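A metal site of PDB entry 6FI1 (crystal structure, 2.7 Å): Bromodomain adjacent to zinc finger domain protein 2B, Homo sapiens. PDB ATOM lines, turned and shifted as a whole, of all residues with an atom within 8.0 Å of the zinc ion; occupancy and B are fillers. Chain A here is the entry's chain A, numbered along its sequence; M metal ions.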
ATOM      1  N   LEU A  23      -7.310 -21.625 -33.474  1.00  0.00           N
ATOM      2  CA  LEU A  23      -7.972 -20.468 -32.866  1.00  0.00           C
ATOM      3  C   LEU A  23      -8.781 -20.981 -31.678  1.00  0.00           C
ATOM      4  O   LEU A  23      -9.648 -21.822 -31.854  1.00  0.00           O
ATOM      5  CB  LEU A  23      -8.918 -19.792 -33.882  1.00  0.00           C
ATOM      6  CG  LEU A  23      -9.429 -18.357 -33.620  1.00  0.00           C
ATOM      7  CD1 LEU A  23      -9.784 -17.684 -34.949  1.00  0.00           C
ATOM      8  CD2 LEU A  23     -10.647 -18.268 -32.688  1.00  0.00           C
ATOM      9  N   CYS A  24      -8.502 -20.485 -30.475  1.00  0.00           N
ATOM     10  CA  CYS A  24      -9.273 -20.906 -29.298  1.00  0.00           C
ATOM     11  C   CYS A  24     -10.621 -20.221 -29.314  1.00  0.00           C
ATOM     12  O   CYS A  24     -10.685 -19.009 -29.344  1.00  0.00           O
ATOM     13  CB  CYS A  24      -8.542 -20.620 -27.986  1.00  0.00           C
ATOM     14  SG  CYS A  24      -9.664 -20.593 -26.562  1.00  0.00           S
ATOM     15  N   ASP A  25     -11.709 -20.996 -29.240  1.00  0.00           N
ATOM     16  CA  ASP A  25     -13.051 -20.396 -29.256  1.00  0.00           C
ATOM     17  C   ASP A  25     -13.524 -19.796 -27.953  1.00  0.00           C
ATOM     18  O   ASP A  25     -14.606 -19.211 -27.922  1.00  0.00           O
ATOM     19  CB  ASP A  25     -14.076 -21.408 -29.746  1.00  0.00           C
ATOM     20  CG  ASP A  25     -13.886 -21.717 -31.197  1.00  0.00           C
ATOM     21  OD1 ASP A  25     -14.211 -20.835 -32.042  1.00  0.00           O
ATOM     22  OD2 ASP A  25     -13.394 -22.818 -31.480  1.00  0.00           O
ATOM     23  N   GLY A  26     -12.741 -19.952 -26.887  1.00  0.00           N
ATOM     24  CA  GLY A  26     -12.940 -19.207 -25.662  1.00  0.00           C
ATOM     25  C   GLY A  26     -12.525 -17.761 -25.826  1.00  0.00           C
ATOM     26  O   GLY A  26     -13.373 -16.858 -25.861  1.00  0.00           O
ATOM     27  N   CYS A  27     -11.218 -17.577 -25.978  1.00  0.00           N
ATOM     28  CA  CYS A  27     -10.547 -16.275 -25.931  1.00  0.00           C
ATOM     29  C   CYS A  27     -10.067 -15.756 -27.284  1.00  0.00           C
ATOM     30  O   CYS A  27      -9.319 -14.784 -27.338  1.00  0.00           O
ATOM     31  CB  CYS A  27      -9.342 -16.417 -25.018  1.00  0.00           C
ATOM     32  SG  CYS A  27      -8.109 -17.546 -25.691  1.00  0.00           S
ATOM     33  N   ASP A  28     -10.473 -16.419 -28.371  1.00  0.00           N
ATOM     34  CA  ASP A  28     -10.046 -16.061 -29.730  1.00  0.00           C
ATOM     35  C   ASP A  28      -8.550 -16.056 -29.993  1.00  0.00           C
ATOM     36  O   ASP A  28      -8.150 -15.477 -30.979  1.00  0.00           O
ATOM     37  CB  ASP A  28     -10.677 -14.725 -30.174  1.00  0.00           C
ATOM     38  CG  ASP A  28     -12.156 -14.858 -30.530  1.00  0.00           C
ATOM     39  OD1 ASP A  28     -12.597 -16.001 -30.832  1.00  0.00           O
ATOM     40  OD2 ASP A  28     -12.858 -13.819 -30.525  1.00  0.00           O
ATOM     41  N   LYS A  29      -7.737 -16.735 -29.188  1.00  0.00           N
ATOM     42  CA  LYS A  29      -6.280 -16.729 -29.401  1.00  0.00           C
ATOM     43  C   LYS A  29      -5.864 -17.911 -30.217  1.00  0.00           C
ATOM     44  O   LYS A  29      -6.546 -18.894 -30.268  1.00  0.00           O
ATOM     45  CB  LYS A  29      -5.498 -16.794 -28.102  1.00  0.00           C
ATOM     46  CG  LYS A  29      -5.340 -15.501 -27.344  1.00  0.00           C
ATOM     47  CD  LYS A  29      -4.527 -15.792 -26.091  1.00  0.00           C
ATOM     48  CE  LYS A  29      -4.360 -14.554 -25.231  1.00  0.00           C
ATOM     49  NZ  LYS A  29      -5.567 -14.309 -24.381  1.00  0.00           N
ATOM     50  N   GLY A  30      -4.677 -17.834 -30.772  1.00  0.00           N
ATOM     51  CA  GLY A  30      -4.193 -18.773 -31.756  1.00  0.00           C
ATOM     52  C   GLY A  30      -2.957 -19.419 -31.224  1.00  0.00           C
ATOM     53  O   GLY A  30      -2.270 -18.857 -30.396  1.00  0.00           O
ATOM     54  N   TRP A  48     -12.074 -25.753 -30.298  1.00  0.00           N
ATOM     55  CA  TRP A  48     -10.822 -25.748 -29.557  1.00  0.00           C
ATOM     56  C   TRP A  48     -10.876 -24.806 -28.346  1.00  0.00           C
ATOM     57  O   TRP A  48     -11.068 -23.596 -28.466  1.00  0.00           O
ATOM     58  CB  TRP A  48      -9.693 -25.314 -30.493  1.00  0.00           C
ATOM     59  CG  TRP A  48      -8.372 -25.184 -29.825  1.00  0.00           C
ATOM     60  CD1 TRP A  48      -7.581 -24.072 -29.717  1.00  0.00           C
ATOM     61  CD2 TRP A  48      -7.689 -26.225 -29.173  1.00  0.00           C
ATOM     62  NE1 TRP A  48      -6.443 -24.361 -29.015  1.00  0.00           N
ATOM     63  CE2 TRP A  48      -6.494 -25.689 -28.671  1.00  0.00           C
ATOM     64  CE3 TRP A  48      -7.979 -27.571 -28.960  1.00  0.00           C
ATOM     65  CZ2 TRP A  48      -5.591 -26.456 -27.958  1.00  0.00           C
ATOM     66  CZ3 TRP A  48      -7.088 -28.330 -28.275  1.00  0.00           C
ATOM     67  CH2 TRP A  48      -5.906 -27.790 -27.788  1.00  0.00           C
ATOM     68  N   PHE A  49     -10.695 -25.358 -27.171  1.00  0.00           N
ATOM     69  CA  PHE A  49     -10.510 -24.535 -26.019  1.00  0.00           C
ATOM     70  C   PHE A  49      -9.069 -24.684 -25.589  1.00  0.00           C
ATOM     71  O   PHE A  49      -8.574 -25.804 -25.408  1.00  0.00           O
ATOM     72  CB  PHE A  49     -11.502 -24.909 -24.972  1.00  0.00           C
ATOM     73  CG  PHE A  49     -12.917 -24.615 -25.388  1.00  0.00           C
ATOM     74  CD1 PHE A  49     -13.445 -23.326 -25.259  1.00  0.00           C
ATOM     75  CD2 PHE A  49     -13.716 -25.612 -25.959  1.00  0.00           C
ATOM     76  CE1 PHE A  49     -14.753 -23.060 -25.656  1.00  0.00           C
ATOM     77  CE2 PHE A  49     -15.011 -25.336 -26.352  1.00  0.00           C
ATOM     78  CZ  PHE A  49     -15.533 -24.054 -26.202  1.00  0.00           C
ATOM     79  N   CYS A  50      -8.400 -23.526 -25.494  1.00  0.00           N
ATOM     80  CA  CYS A  50      -6.987 -23.425 -25.183  1.00  0.00           C
ATOM     81  C   CYS A  50      -6.788 -23.882 -23.750  1.00  0.00           C
ATOM     82  O   CYS A  50      -7.734 -23.892 -22.958  1.00  0.00           O
ATOM     83  CB  CYS A  50      -6.457 -21.996 -25.362  1.00  0.00           C
ATOM     84  SG  CYS A  50      -6.769 -20.871 -23.975  1.00  0.00           S
ATOM     85  N   PRO A  51      -5.548 -24.264 -23.404  1.00  0.00           N
ATOM     86  CA  PRO A  51      -5.256 -24.740 -22.047  1.00  0.00           C
ATOM     87  C   PRO A  51      -5.668 -23.752 -20.937  1.00  0.00           C
ATOM     88  O   PRO A  51      -6.174 -24.169 -19.894  1.00  0.00           O
ATOM     89  CB  PRO A  51      -3.731 -24.921 -22.066  1.00  0.00           C
ATOM     90  CG  PRO A  51      -3.327 -24.917 -23.510  1.00  0.00           C
ATOM     91  CD  PRO A  51      -4.327 -24.078 -24.211  1.00  0.00           C
ATOM     92  N   ALA A  52      -5.459 -22.459 -21.172  1.00  0.00           N
ATOM     93  CA  ALA A  52      -5.793 -21.421 -20.190  1.00  0.00           C
ATOM     94  C   ALA A  52      -7.285 -21.371 -19.930  1.00  0.00           C
ATOM     95  O   ALA A  52      -7.702 -21.262 -18.792  1.00  0.00           O
ATOM     96  CB  ALA A  52      -5.297 -20.044 -20.628  1.00  0.00           C
ATOM     97  N   CYS A  53      -8.066 -21.476 -21.010  1.00  0.00           N
ATOM     98  CA  CYS A  53      -9.527 -21.414 -20.902  1.00  0.00           C
ATOM     99  C   CYS A  53     -10.126 -22.586 -20.093  1.00  0.00           C
ATOM    100  O   CYS A  53     -11.055 -22.392 -19.304  1.00  0.00           O
ATOM    101  CB  CYS A  53     -10.156 -21.306 -22.290  1.00  0.00           C
ATOM    102  SG  CYS A  53     -10.070 -19.614 -22.918  1.00  0.00           S
ATOM    103  N   ILE A  54      -9.532 -23.762 -20.254  1.00  0.00           N
ATOM    104  CA  ILE A  54     -10.003 -24.986 -19.606  1.00  0.00           C
ATOM    105  C   ILE A  54      -9.818 -24.939 -18.098  1.00  0.00           C
ATOM    106  O   ILE A  54     -10.729 -25.314 -17.377  1.00  0.00           O
ATOM    107  CB  ILE A  54      -9.262 -26.234 -20.144  1.00  0.00           C
ATOM    108  CG1 ILE A  54      -9.537 -26.437 -21.650  1.00  0.00           C
ATOM    109  CG2 ILE A  54      -9.643 -27.487 -19.351  1.00  0.00           C
ATOM    110  CD1 ILE A  54     -10.974 -26.775 -22.014  1.00  0.00           C
ATOM    111  N   LYS A  56      -9.782 -22.310 -16.313  1.00  0.00           N
ATOM    112  CA  LYS A  56     -10.825 -21.387 -15.827  1.00  0.00           C
ATOM    113  C   LYS A  56     -12.173 -22.101 -15.747  1.00  0.00           C
ATOM    114  O   LYS A  56     -12.878 -22.006 -14.734  1.00  0.00           O
ATOM    115  CB  LYS A  56     -10.993 -20.175 -16.761  1.00  0.00           C
ATOM    116  CG  LYS A  56      -9.705 -19.524 -17.233  1.00  0.00           C
ATOM    117  CD  LYS A  56      -9.872 -18.038 -17.444  1.00  0.00           C
ATOM    118  CE  LYS A  56      -8.559 -17.394 -17.857  1.00  0.00           C
ATOM    119  NZ  LYS A  56      -8.122 -17.808 -19.218  1.00  0.00           N
HETATM  120 ZN    ZN M   1      -8.574 -19.598 -24.720  1.00  0.00          ZN
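SG of Cys 24 lies close to N of Gly 26 (3.2 Å). SG of Cys 50 sits close to N of Ala 52, 3.5 Å away. N of Lys 29 sits close to SG of Cys 27 (3.6 Å). The backbone carbonyl oxygen of Lys 29 is in hydrogen-bond range of the backbone NH of Cys 24 (2.5 Å).
Along chain A the residues within 4 Å of the zinc ion span positions 24 to 53.
The zinc ion is bound by SG of Cys 27, 2.3 Å away. The side-chain sulfur (SG) of Cys 50 is bound to the zinc ion, at 2.3 Å. SG of Cys 53 binds the zinc ion (2.3 Å). The zinc ion is bound by the side-chain sulfur (SG) of Cys 24. The zinc ion has four donor atoms within binding distance.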
